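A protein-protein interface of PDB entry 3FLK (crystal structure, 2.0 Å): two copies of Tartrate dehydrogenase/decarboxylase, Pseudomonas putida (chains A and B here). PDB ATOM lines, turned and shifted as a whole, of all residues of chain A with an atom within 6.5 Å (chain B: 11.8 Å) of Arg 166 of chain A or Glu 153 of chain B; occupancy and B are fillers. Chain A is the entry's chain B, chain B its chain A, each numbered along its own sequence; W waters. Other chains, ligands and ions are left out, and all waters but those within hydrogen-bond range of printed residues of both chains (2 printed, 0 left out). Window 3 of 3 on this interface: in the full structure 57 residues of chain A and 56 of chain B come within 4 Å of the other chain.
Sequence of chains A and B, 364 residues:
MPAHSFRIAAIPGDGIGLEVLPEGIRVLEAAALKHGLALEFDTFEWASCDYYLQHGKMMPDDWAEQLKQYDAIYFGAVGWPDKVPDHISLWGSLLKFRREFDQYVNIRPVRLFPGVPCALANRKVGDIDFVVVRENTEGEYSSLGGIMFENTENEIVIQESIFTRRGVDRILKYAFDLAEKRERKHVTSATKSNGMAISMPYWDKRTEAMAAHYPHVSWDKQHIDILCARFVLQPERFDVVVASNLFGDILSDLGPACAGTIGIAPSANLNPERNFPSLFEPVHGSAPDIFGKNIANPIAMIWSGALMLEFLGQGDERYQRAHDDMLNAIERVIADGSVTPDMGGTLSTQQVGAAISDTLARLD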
ATOM      1  N   GLU A 138     -17.404  29.857   4.420  1.00  0.00           N
ATOM      2  CA  GLU A 138     -16.674  29.827   3.148  1.00  0.00           C
ATOM      3  C   GLU A 138     -17.173  28.701   2.242  1.00  0.00           C
ATOM      4  O   GLU A 138     -18.336  28.313   2.321  1.00  0.00           O
ATOM      5  CB  GLU A 138     -15.151  29.744   3.381  1.00  0.00           C
ATOM      6  CG  GLU A 138     -14.691  28.585   4.271  1.00  0.00           C
ATOM      7  CD  GLU A 138     -13.179  28.490   4.414  1.00  0.00           C
ATOM      8  OE1 GLU A 138     -12.636  27.386   4.198  1.00  0.00           O
ATOM      9  OE2 GLU A 138     -12.533  29.508   4.745  1.00  0.00           O
ATOM     10  N   THR A 164      -9.969  27.941   3.062  1.00  0.00           N
ATOM     11  CA  THR A 164      -8.744  28.377   3.733  1.00  0.00           C
ATOM     12  C   THR A 164      -8.356  27.356   4.795  1.00  0.00           C
ATOM     13  O   THR A 164      -9.224  26.671   5.333  1.00  0.00           O
ATOM     14  CB  THR A 164      -8.915  29.762   4.404  1.00  0.00           C
ATOM     15  OG1 THR A 164      -9.902  29.680   5.443  1.00  0.00           O
ATOM     16  CG2 THR A 164      -9.333  30.821   3.380  1.00  0.00           C
ATOM     17  N   ARG A 165      -7.064  27.252   5.098  1.00  0.00           N
ATOM     18  CA  ARG A 165      -6.612  26.356   6.167  1.00  0.00           C
ATOM     19  C   ARG A 165      -7.291  26.703   7.488  1.00  0.00           C
ATOM     20  O   ARG A 165      -7.758  25.815   8.199  1.00  0.00           O
ATOM     21  CB  ARG A 165      -5.088  26.372   6.331  1.00  0.00           C
ATOM     22  CG  ARG A 165      -4.602  25.483   7.478  1.00  0.00           C
ATOM     23  CD  ARG A 165      -3.095  25.420   7.583  1.00  0.00           C
ATOM     24  NE  ARG A 165      -2.515  24.585   6.537  1.00  0.00           N
ATOM     25  CZ  ARG A 165      -1.377  23.911   6.656  1.00  0.00           C
ATOM     26  NH1 ARG A 165      -0.685  23.952   7.790  1.00  0.00           N
ATOM     27  NH2 ARG A 165      -0.934  23.185   5.641  1.00  0.00           N
ATOM     28  N   ARG A 166      -7.348  27.998   7.800  1.00  0.00           N
ATOM     29  CA  ARG A 166      -7.995  28.475   9.017  1.00  0.00           C
ATOM     30  C   ARG A 166      -9.444  27.996   9.111  1.00  0.00           C
ATOM     31  O   ARG A 166      -9.856  27.458  10.139  1.00  0.00           O
ATOM     32  CB  ARG A 166      -7.933  30.004   9.107  1.00  0.00           C
ATOM     33  CG  ARG A 166      -6.541  30.545   9.429  1.00  0.00           C
ATOM     34  CD  ARG A 166      -6.576  32.029   9.756  1.00  0.00           C
ATOM     35  NE  ARG A 166      -5.244  32.550  10.066  1.00  0.00           N
ATOM     36  CZ  ARG A 166      -4.407  33.072   9.170  1.00  0.00           C
ATOM     37  NH1 ARG A 166      -4.749  33.150   7.890  1.00  0.00           N
ATOM     38  NH2 ARG A 166      -3.220  33.519   9.558  1.00  0.00           N
ATOM     39  N   GLY A 167     -10.198  28.183   8.029  1.00  0.00           N
ATOM     40  CA  GLY A 167     -11.614  27.818   7.985  1.00  0.00           C
ATOM     41  C   GLY A 167     -11.852  26.319   7.997  1.00  0.00           C
ATOM     42  O   GLY A 167     -12.749  25.832   8.688  1.00  0.00           O
ATOM     43  N   VAL A 168     -11.050  25.589   7.227  1.00  0.00           N
ATOM     44  CA  VAL A 168     -11.170  24.133   7.145  1.00  0.00           C
ATOM     45  C   VAL A 168     -10.765  23.480   8.476  1.00  0.00           C
ATOM     46  O   VAL A 168     -11.483  22.626   8.995  1.00  0.00           O
ATOM     47  CB  VAL A 168     -10.376  23.554   5.940  1.00  0.00           C
ATOM     48  CG1 VAL A 168     -10.376  22.032   5.961  1.00  0.00           C
ATOM     49  CG2 VAL A 168     -10.970  24.053   4.626  1.00  0.00           C
ATOM     50  N   ASP A 169      -9.639  23.911   9.040  1.00  0.00           N
ATOM     51  CA  ASP A 169      -9.168  23.360  10.315  1.00  0.00           C
ATOM     52  C   ASP A 169     -10.145  23.561  11.474  1.00  0.00           C
ATOM     53  O   ASP A 169     -10.392  22.626  12.235  1.00  0.00           O
ATOM     54  CB  ASP A 169      -7.781  23.900  10.679  1.00  0.00           C
ATOM     55  CG  ASP A 169      -6.666  23.249   9.873  1.00  0.00           C
ATOM     56  OD1 ASP A 169      -6.956  22.435   8.963  1.00  0.00           O
ATOM     57  OD2 ASP A 169      -5.488  23.555  10.154  1.00  0.00           O
ATOM     58  N   ARG A 170     -10.714  24.760  11.599  1.00  0.00           N
ATOM     59  CA  ARG A 170     -11.600  25.050  12.730  1.00  0.00           C
ATOM     60  C   ARG A 170     -12.914  24.260  12.707  1.00  0.00           C
ATOM     61  O   ARG A 170     -13.408  23.867  13.763  1.00  0.00           O
ATOM     62  CB  ARG A 170     -11.848  26.555  12.912  1.00  0.00           C
ATOM     63  CG  ARG A 170     -12.573  27.243  11.769  1.00  0.00           C
ATOM     64  CD  ARG A 170     -12.679  28.737  12.025  1.00  0.00           C
ATOM     65  NE  ARG A 170     -13.459  29.408  10.983  1.00  0.00           N
ATOM     66  CZ  ARG A 170     -13.723  30.713  10.962  1.00  0.00           C
ATOM     67  NH1 ARG A 170     -13.276  31.510  11.928  1.00  0.00           N
ATOM     68  NH2 ARG A 170     -14.441  31.222   9.970  1.00  0.00           N
ATOM     69  N   ILE A 171     -13.467  24.016  11.519  1.00  0.00           N
ATOM     70  CA  ILE A 171     -14.693  23.211  11.425  1.00  0.00           C
ATOM     71  C   ILE A 171     -14.403  21.729  11.698  1.00  0.00           C
ATOM     72  O   ILE A 171     -15.176  21.057  12.383  1.00  0.00           O
ATOM     73  CB  ILE A 171     -15.480  23.434  10.086  1.00  0.00           C
ATOM     74  CG1 ILE A 171     -16.896  22.844  10.171  1.00  0.00           C
ATOM     75  CG2 ILE A 171     -14.727  22.870   8.880  1.00  0.00           C
ATOM     76  CD1 ILE A 171     -17.854  23.617  11.073  1.00  0.00           C
ATOM     77  N   TYR A 202      -7.896  18.709  -1.060  1.00  0.00           N
ATOM     78  CA  TYR A 202      -7.378  19.548   0.019  1.00  0.00           C
ATOM     79  C   TYR A 202      -8.140  19.320   1.327  1.00  0.00           C
ATOM     80  O   TYR A 202      -7.532  19.158   2.386  1.00  0.00           O
ATOM     81  CB  TYR A 202      -7.417  21.031  -0.360  1.00  0.00           C
ATOM     82  CG  TYR A 202      -6.970  21.925   0.770  1.00  0.00           C
ATOM     83  CD1 TYR A 202      -5.619  22.055   1.078  1.00  0.00           C
ATOM     84  CD2 TYR A 202      -7.897  22.622   1.544  1.00  0.00           C
ATOM     85  CE1 TYR A 202      -5.198  22.865   2.119  1.00  0.00           C
ATOM     86  CE2 TYR A 202      -7.486  23.435   2.594  1.00  0.00           C
ATOM     87  CZ  TYR A 202      -6.132  23.553   2.870  1.00  0.00           C
ATOM     88  OH  TYR A 202      -5.711  24.353   3.898  1.00  0.00           O
ATOM     89  N   ILE B 147      -3.579  26.525  -5.214  1.00  0.00           N
ATOM     90  CA  ILE B 147      -3.269  26.782  -3.812  1.00  0.00           C
ATOM     91  C   ILE B 147      -2.271  27.935  -3.653  1.00  0.00           C
ATOM     92  O   ILE B 147      -1.290  28.027  -4.394  1.00  0.00           O
ATOM     93  CB  ILE B 147      -2.771  25.484  -3.103  1.00  0.00           C
ATOM     94  CG1 ILE B 147      -2.572  25.711  -1.598  1.00  0.00           C
ATOM     95  CG2 ILE B 147      -1.507  24.932  -3.783  1.00  0.00           C
ATOM     96  CD1 ILE B 147      -2.603  24.425  -0.780  1.00  0.00           C
ATOM     97  N   MET B 148      -2.550  28.813  -2.694  1.00  0.00           N
ATOM     98  CA  MET B 148      -1.671  29.929  -2.347  1.00  0.00           C
ATOM     99  C   MET B 148      -1.189  29.778  -0.914  1.00  0.00           C
ATOM    100  O   MET B 148      -1.937  29.314  -0.055  1.00  0.00           O
ATOM    101  CB  MET B 148      -2.412  31.264  -2.473  1.00  0.00           C
ATOM    102  CG  MET B 148      -2.571  31.769  -3.890  1.00  0.00           C
ATOM    103  SD  MET B 148      -0.885  32.366  -4.665  1.00  0.00           S
ATOM    104  CE  MET B 148      -0.705  34.080  -3.745  1.00  0.00           C
ATOM    105  N   PHE B 149       0.053  30.194  -0.667  1.00  0.00           N
ATOM    106  CA  PHE B 149       0.668  30.164   0.668  1.00  0.00           C
ATOM    107  C   PHE B 149       0.657  28.758   1.272  1.00  0.00           C
ATOM    108  O   PHE B 149       0.415  28.585   2.470  1.00  0.00           O
ATOM    109  CB  PHE B 149      -0.010  31.168   1.614  1.00  0.00           C
ATOM    110  CG  PHE B 149      -0.304  32.505   0.983  1.00  0.00           C
ATOM    111  CD1 PHE B 149       0.732  33.333   0.552  1.00  0.00           C
ATOM    112  CD2 PHE B 149      -1.617  32.939   0.827  1.00  0.00           C
ATOM    113  CE1 PHE B 149       0.461  34.573  -0.035  1.00  0.00           C
ATOM    114  CE2 PHE B 149      -1.900  34.179   0.245  1.00  0.00           C
ATOM    115  CZ  PHE B 149      -0.856  34.997  -0.185  1.00  0.00           C
ATOM    116  N   GLU B 150       0.929  27.764   0.427  1.00  0.00           N
ATOM    117  CA  GLU B 150       0.880  26.353   0.812  1.00  0.00           C
ATOM    118  C   GLU B 150       1.741  26.064   2.040  1.00  0.00           C
ATOM    119  O   GLU B 150       2.835  26.619   2.187  1.00  0.00           O
ATOM    120  CB  GLU B 150       1.309  25.465  -0.360  1.00  0.00           C
ATOM    121  CG  GLU B 150       1.021  23.976  -0.169  1.00  0.00           C
ATOM    122  CD  GLU B 150       1.344  23.137  -1.398  1.00  0.00           C
ATOM    123  OE1 GLU B 150       1.885  23.680  -2.388  1.00  0.00           O
ATOM    124  OE2 GLU B 150       1.055  21.920  -1.373  1.00  0.00           O
ATOM    125  N   ASN B 151       1.219  25.207   2.917  1.00  0.00           N
ATOM    126  CA  ASN B 151       1.914  24.757   4.132  1.00  0.00           C
ATOM    127  C   ASN B 151       2.124  25.841   5.196  1.00  0.00           C
ATOM    128  O   ASN B 151       2.981  25.700   6.070  1.00  0.00           O
ATOM    129  CB  ASN B 151       3.242  24.062   3.785  1.00  0.00           C
ATOM    130  CG  ASN B 151       3.053  22.835   2.905  1.00  0.00           C
ATOM    131  OD1 ASN B 151       2.119  22.053   3.094  1.00  0.00           O
ATOM    132  ND2 ASN B 151       3.947  22.661   1.941  1.00  0.00           N
ATOM    133  N   THR B 152       1.340  26.915   5.117  1.00  0.00           N
ATOM    134  CA  THR B 152       1.359  27.976   6.129  1.00  0.00           C
ATOM    135  C   THR B 152      -0.050  28.230   6.668  1.00  0.00           C
ATOM    136  O   THR B 152      -1.034  27.763   6.096  1.00  0.00           O
ATOM    137  CB  THR B 152       1.951  29.319   5.590  1.00  0.00           C
ATOM    138  OG1 THR B 152       0.998  29.977   4.743  1.00  0.00           O
ATOM    139  CG2 THR B 152       3.257  29.100   4.828  1.00  0.00           C
ATOM    140  N   GLU B 153      -0.131  28.976   7.766  1.00  0.00           N
ATOM    141  CA  GLU B 153      -1.401  29.366   8.374  1.00  0.00           C
ATOM    142  C   GLU B 153      -2.290  30.171   7.407  1.00  0.00           C
ATOM    143  O   GLU B 153      -3.513  30.187   7.548  1.00  0.00           O
ATOM    144  CB  GLU B 153      -1.127  30.168   9.655  1.00  0.00           C
ATOM    145  CG  GLU B 153      -2.313  30.327  10.606  1.00  0.00           C
ATOM    146  CD  GLU B 153      -1.957  31.102  11.876  1.00  0.00           C
ATOM    147  OE1 GLU B 153      -1.355  32.199  11.776  1.00  0.00           O
ATOM    148  OE2 GLU B 153      -2.286  30.619  12.981  1.00  0.00           O
ATOM    149  N   ASN B 154      -1.663  30.821   6.426  1.00  0.00           N
ATOM    150  CA  ASN B 154      -2.358  31.682   5.464  1.00  0.00           C
ATOM    151  C   ASN B 154      -2.818  30.949   4.202  1.00  0.00           C
ATOM    152  O   ASN B 154      -3.328  31.568   3.269  1.00  0.00           O
ATOM    153  CB  ASN B 154      -1.465  32.870   5.080  1.00  0.00           C
ATOM    154  CG  ASN B 154      -1.097  33.736   6.271  1.00  0.00           C
ATOM    155  OD1 ASN B 154      -1.946  34.070   7.097  1.00  0.00           O
ATOM    156  ND2 ASN B 154       0.174  34.107   6.362  1.00  0.00           N
ATOM    157  N   GLU B 155      -2.627  29.632   4.191  1.00  0.00           N
ATOM    158  CA  GLU B 155      -2.973  28.764   3.066  1.00  0.00           C
ATOM    159  C   GLU B 155      -4.402  28.991   2.553  1.00  0.00           C
ATOM    160  O   GLU B 155      -5.360  28.959   3.325  1.00  0.00           O
ATOM    161  CB  GLU B 155      -2.785  27.307   3.490  1.00  0.00           C
ATOM    162  CG  GLU B 155      -2.853  26.272   2.388  1.00  0.00           C
ATOM    163  CD  GLU B 155      -2.434  24.899   2.889  1.00  0.00           C
ATOM    164  OE1 GLU B 155      -3.062  24.390   3.843  1.00  0.00           O
ATOM    165  OE2 GLU B 155      -1.464  24.336   2.343  1.00  0.00           O
ATOM    166  N   ILE B 156      -4.513  29.232   1.248  1.00  0.00           N
ATOM    167  CA  ILE B 156      -5.796  29.457   0.567  1.00  0.00           C
ATOM    168  C   ILE B 156      -5.909  28.513  -0.627  1.00  0.00           C
ATOM    169  O   ILE B 156      -4.945  28.328  -1.373  1.00  0.00           O
ATOM    170  CB  ILE B 156      -5.933  30.926   0.059  1.00  0.00           C
ATOM    171  CG1 ILE B 156      -5.857  31.922   1.218  1.00  0.00           C
ATOM    172  CG2 ILE B 156      -7.247  31.132  -0.713  1.00  0.00           C
ATOM    173  CD1 ILE B 156      -5.446  33.332   0.782  1.00  0.00           C
ATOM    174  N   VAL B 157      -7.091  27.929  -0.803  1.00  0.00           N
ATOM    175  CA  VAL B 157      -7.375  27.052  -1.936  1.00  0.00           C
ATOM    176  C   VAL B 157      -8.558  27.608  -2.734  1.00  0.00           C
ATOM    177  O   VAL B 157      -9.616  27.891  -2.172  1.00  0.00           O
ATOM    178  CB  VAL B 157      -7.653  25.600  -1.474  1.00  0.00           C
ATOM    179  CG1 VAL B 157      -8.211  24.751  -2.611  1.00  0.00           C
ATOM    180  CG2 VAL B 157      -6.379  24.970  -0.927  1.00  0.00           C
HETATM  181  O   HOH W   1      -5.684  30.223   5.914  1.00  0.00           O
HETATM  182  O   HOH W   2       1.302  21.396   5.597  1.00  0.00           O
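The side-chain carboxylate (OE1) of Glu 153 of chain B is in salt-bridge range of the guanidinium group (NH2) of Arg 166 of chain A. The side-chain carboxylate of Glu 155 of chain B is in hydrogen-bond range of the side-chain hydroxyl of Tyr 202 of chain A, 2.6 Å away. The side-chain carboxylate (OE1) of Glu 155 of chain B lies within salt-bridge range of the guanidinium group (NE) of Arg 165 of chain A (2.8 Å). The side-chain amide oxygen (OD1) of Asn 154 of chain B sits at hydrogen-bond distance from the guanidinium group (NH2) of Arg 166 of chain A (2.8 Å).
OG1 of Thr 164 of chain A is in hydrogen-bond range of OE2 of Glu 138 of chain A (2.7 Å). The backbone NH (N) of Arg 165 of chain A sits close to the side-chain hydroxyl (OH) of Tyr 202 of chain A (3.4 Å). OG1 of Thr 164 of chain A sits at hydrogen-bond distance from N of Gly 167 of chain A (3.0 Å). N of Asn 151 of chain B sits at hydrogen-bond distance from OE2 of Glu 155 of chain B. The side-chain hydroxyl (OG1) of Thr 152 of chain B lies within hydrogen-bond range of the backbone carbonyl oxygen (O) of Phe 149 of chain B (2.7 Å). OG1 of Thr 152 of chain B lies close to N of Asn 154 of chain B, at 3.3 Å.
Among the printed residues, merely in contact across the chains: Thr 164 of chain A with Glu 155 of chain B (3.5 Å), Arg 165 of chain A with Asn 151 of chain B (3.6 Å), Arg 165 of chain A with Thr 152 of chain B (3.5 Å) and Tyr 202 of chain A with Val 157 of chain B (3.5 Å).
Printed residues of chain B within 4 Å of Arg 166 of chain A: Glu 153 (3.2 Å) and Asn 154 (2.8 Å). Of chain A, only Arg 166 (3.2 Å) comes within 4 Å of Glu 153 of chain B. Thr 164 of chain A touches one residue of chain B. Of chain B, only Asn 151, Thr 152 and Glu 155 come within 4 Å of Arg 165 of chain A. No residue of chain B comes within 4 Å of Val 168 of chain A. No residue of chain B comes within 4 Å of Asp 169 of chain A. No residue of chain B comes within 4 Å of Arg 170 of chain A. Of the printed residues of chain A, Asn 154 of chain B touches Arg 166 (2.8 Å). Printed residues of chain A within 4 Å of Thr 152 of chain B: Arg 165 (3.5 Å). Glu 150 of chain B touches none of the printed residues of chain A. The nearest residue of chain A that does not touch Glu 153 of chain B is Arg 165 of chain A (4.3 Å). The nearest printed residue of chain A that does not touch Val 157 of chain B is Thr 164 of chain A (4.8 Å).
Of the 10 printed residues of chain A, 4 touch a printed residue of chain B. Hydrophobic or aromatic side chains of chain A within 4 Å of the printed part of chain B: Tyr 202. Printed residues of chain B that touch a printed residue of chain A: Asn 151, Thr 152, Glu 153, Asn 154, Glu 155 and Val 157. Hydrophobic or aromatic side chains of chain B that line the printed part of chain A: Val 157. Among the printed residues, 8 pairs touch across the chains. Among the printed residues, Asp or Glu carboxylates within 4 Å of a Lys or Arg side-chain nitrogen of the other chain: Arg 165 of chain A with Glu 155 of chain B and Arg 166 of chain A with Glu 153 of chain B.
No position is printed for both chains. Of the 8 pairs that touch across the chains among the printed residues, none has its exchanged pair printed and touching as well.
Water W2 bridges the side-chain amide oxygen (OD1) of Asn 151 of chain B (2.7 Å) and the guanidinium group (NH2) of Arg 165 of chain A (2.9 Å). Water W1 lies within hydrogen-bond range of the backbone carbonyl oxygen (O) of Glu 153 of chain B (2.7 Å), the backbone carbonyl oxygen (O) of Glu 155 of chain B (2.9 Å), the backbone NH (N) of Arg 166 of chain A (3.4 Å) and the backbone NH (N) of Arg 165 of chain A (3.4 Å).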
